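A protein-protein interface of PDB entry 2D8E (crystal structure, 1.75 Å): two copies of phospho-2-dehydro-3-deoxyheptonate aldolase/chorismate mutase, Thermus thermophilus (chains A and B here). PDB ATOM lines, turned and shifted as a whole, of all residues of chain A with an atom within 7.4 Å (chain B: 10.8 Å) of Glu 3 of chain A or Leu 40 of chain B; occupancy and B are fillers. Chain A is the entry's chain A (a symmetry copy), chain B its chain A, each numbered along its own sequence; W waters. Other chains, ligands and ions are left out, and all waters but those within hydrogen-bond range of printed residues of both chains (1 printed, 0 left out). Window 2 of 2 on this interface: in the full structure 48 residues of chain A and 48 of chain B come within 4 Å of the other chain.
The backbone NH (N) of Glu 3 of chain A sits at hydrogen-bond distance from the side-chain amide oxygen (OE1) of Gln 6 of chain A (2.5 Å). The side-chain amide oxygen (OE1) of Gln 37 of chain B sits close to the backbone carbonyl oxygen (O) of Pro 43 of chain B (3.4 Å). NE2 of Gln 37 of chain B lies within hydrogen-bond range of ND1 of His 44 of chain B, 2.9 Å away. O of Gln 37 of chain B is in hydrogen-bond range of N of Leu 42 of chain B, 2.7 Å away.
Among the printed residues, merely in contact across the chains: Glu 3 of chain A with Leu 40 of chain B (3.8 Å), Arg 4 of chain A with Leu 36 of chain B (3.6 Å), Ile 5 of chain A with Leu 36 of chain B (3.9 Å), Ile 5 of chain A with Gln 37 of chain B (3.9 Å), Ile 5 of chain A with Leu 42 of chain B (3.5 Å), Leu 8 of chain A with Glu 32 of chain B (3.4 Å), Leu 8 of chain A with Ile 33 of chain B (3.5 Å) and Leu 8 of chain A with Leu 36 of chain B (3.4 Å).
Of chain B, only Leu 40 (3.8 Å) comes within 4 Å of Glu 3 of chain A. Ile 5 of chain A touches three residues of chain B. No residue of chain B comes within 4 Å of Gln 6 of chain A. No residue of chain B comes within 4 Å of Ala 7 of chain A. Printed residues of chain A within 4 Å of Glu 32 of chain B: Leu 8. Of the printed residues of chain A, Ile 33 of chain B touches Leu 8. Printed residues of chain A within 4 Å of Leu 36 of chain B: Arg 4, Ile 5 and Leu 8. The nearest residue of chain A that does not touch Leu 40 of chain B is Ile 5 of chain A (4.05 Å).
Of the 13 printed residues of chain B, 6 touch a printed residue of chain A. Printed residues of chain B that touch a printed residue of chain A: Glu 32, Ile 33, Leu 36, Gln 37, Leu 40 and Leu 42. Printed residues of chain A that touch a printed residue of chain B: Glu 3, Arg 4, Ile 5 and Leu 8. Along chain A the printed residues that touch a printed residue of chain B span positions 3 to 8.
No position is printed for both chains. Of the 8 pairs that touch across the chains among the printed residues, none has its exchanged pair printed and touching as well.
Water W1 lies within hydrogen-bond range of O of His 44 of chain B (3.0 Å), OE1 of Gln 37 of chain B (3.1 Å) and NH2 of Arg 9 of chain A (3.4 Å).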
ATOM      1  N   GLU A   3     -15.401  -6.538  25.703  1.00  0.00           N
ATOM      2  CA  GLU A   3     -16.186  -7.640  25.077  1.00  0.00           C
ATOM      3  C   GLU A   3     -15.284  -8.798  24.664  1.00  0.00           C
ATOM      4  O   GLU A   3     -14.174  -8.948  25.180  1.00  0.00           O
ATOM      5  CB  GLU A   3     -16.947  -7.109  23.863  1.00  0.00           C
ATOM      6  CG  GLU A   3     -16.067  -6.395  22.846  1.00  0.00           C
ATOM      7  CD  GLU A   3     -16.876  -5.731  21.747  1.00  0.00           C
ATOM      8  OE1 GLU A   3     -17.453  -6.455  20.906  1.00  0.00           O
ATOM      9  OE2 GLU A   3     -16.936  -4.484  21.730  1.00  0.00           O
ATOM     10  N   ARG A   4     -15.770  -9.629  23.745  1.00  0.00           N
ATOM     11  CA  ARG A   4     -14.995 -10.763  23.279  1.00  0.00           C
ATOM     12  C   ARG A   4     -13.737 -10.293  22.559  1.00  0.00           C
ATOM     13  O   ARG A   4     -12.651 -10.831  22.734  1.00  0.00           O
ATOM     14  CB  ARG A   4     -15.868 -11.578  22.324  1.00  0.00           C
ATOM     15  CG  ARG A   4     -16.903 -12.427  23.063  1.00  0.00           C
ATOM     16  CD  ARG A   4     -17.593 -13.431  22.134  1.00  0.00           C
ATOM     17  NE  ARG A   4     -18.701 -14.096  22.826  1.00  0.00           N
ATOM     18  CZ  ARG A   4     -18.450 -15.299  23.377  1.00  0.00           C
ATOM     19  NH1 ARG A   4     -17.245 -15.832  23.288  1.00  0.00           N
ATOM     20  NH2 ARG A   4     -19.427 -15.947  24.018  1.00  0.00           N
ATOM     21  N   ILE A   5     -13.876  -9.267  21.729  1.00  0.00           N
ATOM     22  CA  ILE A   5     -12.721  -8.747  21.011  1.00  0.00           C
ATOM     23  C   ILE A   5     -11.717  -8.150  21.995  1.00  0.00           C
ATOM     24  O   ILE A   5     -10.509  -8.344  21.861  1.00  0.00           O
ATOM     25  CB  ILE A   5     -13.133  -7.673  19.976  1.00  0.00           C
ATOM     26  CG1 ILE A   5     -13.930  -8.327  18.840  1.00  0.00           C
ATOM     27  CG2 ILE A   5     -11.893  -6.989  19.411  1.00  0.00           C
ATOM     28  CD1 ILE A   5     -14.417  -7.347  17.778  1.00  0.00           C
ATOM     29  N   GLN A   6     -12.211  -7.429  22.996  1.00  0.00           N
ATOM     30  CA  GLN A   6     -11.352  -6.837  24.008  1.00  0.00           C
ATOM     31  C   GLN A   6     -10.566  -7.914  24.749  1.00  0.00           C
ATOM     32  O   GLN A   6      -9.384  -7.770  25.034  1.00  0.00           O
ATOM     33  CB  GLN A   6     -12.234  -6.067  24.991  1.00  0.00           C
ATOM     34  CG  GLN A   6     -12.814  -4.791  24.380  1.00  0.00           C
ATOM     35  CD  GLN A   6     -13.450  -3.957  25.467  1.00  0.00           C
ATOM     36  OE1 GLN A   6     -14.161  -4.430  26.337  1.00  0.00           O
ATOM     37  NE2 GLN A   6     -13.163  -2.642  25.380  1.00  0.00           N
ATOM     38  N   ALA A   7     -11.264  -8.996  25.082  1.00  0.00           N
ATOM     39  CA  ALA A   7     -10.652 -10.099  25.813  1.00  0.00           C
ATOM     40  C   ALA A   7      -9.566 -10.746  24.958  1.00  0.00           C
ATOM     41  O   ALA A   7      -8.463 -11.007  25.432  1.00  0.00           O
ATOM     42  CB  ALA A   7     -11.705 -11.132  26.180  1.00  0.00           C
ATOM     43  N   LEU A   8      -9.891 -11.003  23.693  1.00  0.00           N
ATOM     44  CA  LEU A   8      -8.945 -11.619  22.769  1.00  0.00           C
ATOM     45  C   LEU A   8      -7.727 -10.731  22.534  1.00  0.00           C
ATOM     46  O   LEU A   8      -6.610 -11.228  22.435  1.00  0.00           O
ATOM     47  CB  LEU A   8      -9.635 -11.934  21.433  1.00  0.00           C
ATOM     48  CG  LEU A   8     -10.567 -13.148  21.452  1.00  0.00           C
ATOM     49  CD1 LEU A   8     -11.514 -13.108  20.257  1.00  0.00           C
ATOM     50  CD2 LEU A   8      -9.733 -14.422  21.439  1.00  0.00           C
ATOM     51  N   ARG A   9      -7.935  -9.422  22.444  1.00  0.00           N
ATOM     52  CA  ARG A   9      -6.806  -8.522  22.235  1.00  0.00           C
ATOM     53  C   ARG A   9      -5.876  -8.566  23.445  1.00  0.00           C
ATOM     54  O   ARG A   9      -4.661  -8.444  23.317  1.00  0.00           O
ATOM     55  CB  ARG A   9      -7.295  -7.101  21.981  1.00  0.00           C
ATOM     56  CG  ARG A   9      -7.862  -6.915  20.582  1.00  0.00           C
ATOM     57  CD  ARG A   9      -8.178  -5.461  20.302  1.00  0.00           C
ATOM     58  NE  ARG A   9      -8.388  -5.222  18.875  1.00  0.00           N
ATOM     59  CZ  ARG A   9      -8.635  -4.026  18.350  1.00  0.00           C
ATOM     60  NH1 ARG A   9      -8.708  -2.959  19.136  1.00  0.00           N
ATOM     61  NH2 ARG A   9      -8.797  -3.896  17.039  1.00  0.00           N
ATOM     62  N   GLU B  32      -9.814 -15.686  15.526  1.00  0.00           N
ATOM     63  CA  GLU B  32     -11.040 -15.540  16.291  1.00  0.00           C
ATOM     64  C   GLU B  32     -11.498 -14.084  16.268  1.00  0.00           C
ATOM     65  O   GLU B  32     -12.681 -13.804  16.089  1.00  0.00           O
ATOM     66  CB  GLU B  32     -10.838 -16.006  17.733  1.00  0.00           C
ATOM     67  CG  GLU B  32     -12.124 -16.000  18.533  1.00  0.00           C
ATOM     68  CD  GLU B  32     -13.151 -16.961  17.965  1.00  0.00           C
ATOM     69  OE1 GLU B  32     -13.173 -18.134  18.389  1.00  0.00           O
ATOM     70  OE2 GLU B  32     -13.927 -16.547  17.081  1.00  0.00           O
ATOM     71  N   ILE B  33     -10.561 -13.159  16.461  1.00  0.00           N
ATOM     72  CA  ILE B  33     -10.886 -11.738  16.433  1.00  0.00           C
ATOM     73  C   ILE B  33     -11.463 -11.407  15.059  1.00  0.00           C
ATOM     74  O   ILE B  33     -12.438 -10.666  14.939  1.00  0.00           O
ATOM     75  CB  ILE B  33      -9.626 -10.874  16.657  1.00  0.00           C
ATOM     76  CG1 ILE B  33      -9.133 -11.051  18.094  1.00  0.00           C
ATOM     77  CG2 ILE B  33      -9.929  -9.403  16.375  1.00  0.00           C
ATOM     78  CD1 ILE B  33      -7.806 -10.376  18.370  1.00  0.00           C
ATOM     79  N   GLY B  34     -10.852 -11.980  14.028  1.00  0.00           N
ATOM     80  CA  GLY B  34     -11.300 -11.737  12.670  1.00  0.00           C
ATOM     81  C   GLY B  34     -12.736 -12.152  12.414  1.00  0.00           C
ATOM     82  O   GLY B  34     -13.486 -11.417  11.769  1.00  0.00           O
ATOM     83  N   ARG B  35     -13.130 -13.322  12.909  1.00  0.00           N
ATOM     84  CA  ARG B  35     -14.493 -13.789  12.690  1.00  0.00           C
ATOM     85  C   ARG B  35     -15.474 -12.886  13.431  1.00  0.00           C
ATOM     86  O   ARG B  35     -16.564 -12.595  12.935  1.00  0.00           O
ATOM     87  CB  ARG B  35     -14.663 -15.242  13.151  1.00  0.00           C
ATOM     88  CG  ARG B  35     -14.932 -15.406  14.634  1.00  0.00           C
ATOM     89  CD  ARG B  35     -15.987 -16.486  14.885  1.00  0.00           C
ATOM     90  NE  ARG B  35     -17.270 -16.151  14.271  1.00  0.00           N
ATOM     91  CZ  ARG B  35     -18.367 -16.898  14.364  1.00  0.00           C
ATOM     92  NH1 ARG B  35     -18.346 -18.033  15.051  1.00  0.00           N
ATOM     93  NH2 ARG B  35     -19.488 -16.515  13.763  1.00  0.00           N
ATOM     94  N   LEU B  36     -15.081 -12.431  14.620  1.00  0.00           N
ATOM     95  CA  LEU B  36     -15.939 -11.550  15.398  1.00  0.00           C
ATOM     96  C   LEU B  36     -16.101 -10.218  14.664  1.00  0.00           C
ATOM     97  O   LEU B  36     -17.202  -9.675  14.586  1.00  0.00           O
ATOM     98  CB  LEU B  36     -15.347 -11.330  16.797  1.00  0.00           C
ATOM     99  CG  LEU B  36     -15.390 -12.555  17.718  1.00  0.00           C
ATOM    100  CD1 LEU B  36     -14.613 -12.272  18.998  1.00  0.00           C
ATOM    101  CD2 LEU B  36     -16.844 -12.904  18.042  1.00  0.00           C
ATOM    102  N   GLN B  37     -15.008  -9.695  14.117  1.00  0.00           N
ATOM    103  CA  GLN B  37     -15.077  -8.434  13.383  1.00  0.00           C
ATOM    104  C   GLN B  37     -15.981  -8.573  12.167  1.00  0.00           C
ATOM    105  O   GLN B  37     -16.746  -7.665  11.851  1.00  0.00           O
ATOM    106  CB  GLN B  37     -13.677  -7.986  12.963  1.00  0.00           C
ATOM    107  CG  GLN B  37     -12.909  -7.405  14.136  1.00  0.00           C
ATOM    108  CD  GLN B  37     -11.433  -7.224  13.871  1.00  0.00           C
ATOM    109  OE1 GLN B  37     -10.767  -6.428  14.549  1.00  0.00           O
ATOM    110  NE2 GLN B  37     -10.902  -7.966  12.910  1.00  0.00           N
ATOM    111  N   THR B  38     -15.886  -9.712  11.490  1.00  0.00           N
ATOM    112  CA  THR B  38     -16.730  -9.967  10.325  1.00  0.00           C
ATOM    113  C   THR B  38     -18.196  -9.968  10.761  1.00  0.00           C
ATOM    114  O   THR B  38     -19.032  -9.275  10.183  1.00  0.00           O
ATOM    115  CB  THR B  38     -16.392 -11.326   9.681  1.00  0.00           C
ATOM    116  OG1 THR B  38     -15.102 -11.252   9.059  1.00  0.00           O
ATOM    117  CG2 THR B  38     -17.427 -11.698   8.634  1.00  0.00           C
ATOM    118  N   GLU B  39     -18.492 -10.740  11.798  1.00  0.00           N
ATOM    119  CA  GLU B  39     -19.845 -10.846  12.329  1.00  0.00           C
ATOM    120  C   GLU B  39     -20.434  -9.503  12.782  1.00  0.00           C
ATOM    121  O   GLU B  39     -21.629  -9.243  12.605  1.00  0.00           O
ATOM    122  CB  GLU B  39     -19.846 -11.831  13.495  1.00  0.00           C
ATOM    123  CG  GLU B  39     -21.202 -12.062  14.111  1.00  0.00           C
ATOM    124  CD  GLU B  39     -21.183 -13.185  15.126  1.00  0.00           C
ATOM    125  OE1 GLU B  39     -20.358 -13.125  16.066  1.00  0.00           O
ATOM    126  OE2 GLU B  39     -21.993 -14.126  14.987  1.00  0.00           O
ATOM    127  N   LEU B  40     -19.586  -8.654  13.354  1.00  0.00           N
ATOM    128  CA  LEU B  40     -20.013  -7.351  13.851  1.00  0.00           C
ATOM    129  C   LEU B  40     -19.857  -6.202  12.857  1.00  0.00           C
ATOM    130  O   LEU B  40     -20.174  -5.057  13.177  1.00  0.00           O
ATOM    131  CB  LEU B  40     -19.242  -7.013  15.125  1.00  0.00           C
ATOM    132  CG  LEU B  40     -19.437  -7.964  16.306  1.00  0.00           C
ATOM    133  CD1 LEU B  40     -18.439  -7.627  17.400  1.00  0.00           C
ATOM    134  CD2 LEU B  40     -20.863  -7.856  16.823  1.00  0.00           C
ATOM    135  N   GLY B  41     -19.365  -6.502  11.661  1.00  0.00           N
ATOM    136  CA  GLY B  41     -19.187  -5.462  10.664  1.00  0.00           C
ATOM    137  C   GLY B  41     -18.107  -4.462  11.035  1.00  0.00           C
ATOM    138  O   GLY B  41     -18.224  -3.274  10.742  1.00  0.00           O
ATOM    139  N   LEU B  42     -17.053  -4.945  11.682  1.00  0.00           N
ATOM    140  CA  LEU B  42     -15.938  -4.097  12.091  1.00  0.00           C
ATOM    141  C   LEU B  42     -14.754  -4.314  11.158  1.00  0.00           C
ATOM    142  O   LEU B  42     -14.576  -5.400  10.610  1.00  0.00           O
ATOM    143  CB  LEU B  42     -15.519  -4.440  13.525  1.00  0.00           C
ATOM    144  CG  LEU B  42     -16.573  -4.264  14.618  1.00  0.00           C
ATOM    145  CD1 LEU B  42     -16.077  -4.882  15.921  1.00  0.00           C
ATOM    146  CD2 LEU B  42     -16.875  -2.782  14.794  1.00  0.00           C
ATOM    147  N   PRO B  43     -13.923  -3.281  10.959  1.00  0.00           N
ATOM    148  CA  PRO B  43     -12.775  -3.470  10.068  1.00  0.00           C
ATOM    149  C   PRO B  43     -11.733  -4.408  10.674  1.00  0.00           C
ATOM    150  O   PRO B  43     -11.659  -4.568  11.894  1.00  0.00           O
ATOM    151  CB  PRO B  43     -12.246  -2.048   9.882  1.00  0.00           C
ATOM    152  CG  PRO B  43     -12.593  -1.390  11.183  1.00  0.00           C
ATOM    153  CD  PRO B  43     -13.998  -1.888  11.438  1.00  0.00           C
ATOM    154  N   HIS B  44     -10.946  -5.036   9.809  1.00  0.00           N
ATOM    155  CA  HIS B  44      -9.896  -5.961  10.212  1.00  0.00           C
ATOM    156  C   HIS B  44      -8.572  -5.194  10.317  1.00  0.00           C
ATOM    157  O   HIS B  44      -7.720  -5.478  11.148  1.00  0.00           O
ATOM    158  CB  HIS B  44      -9.759  -7.105   9.175  1.00  0.00           C
ATOM    159  CG  HIS B  44     -10.988  -8.011   9.090  1.00  0.00           C
ATOM    160  ND1 HIS B  44     -11.538  -8.650  10.151  1.00  0.00           N
ATOM    161  CD2 HIS B  44     -11.746  -8.303   7.953  1.00  0.00           C
ATOM    162  CE1 HIS B  44     -12.607  -9.308   9.658  1.00  0.00           C
ATOM    163  NE2 HIS B  44     -12.754  -9.118   8.345  1.00  0.00           N
HETATM  164  O   HOH W   1      -7.879  -5.368  14.125  1.00  0.00           O
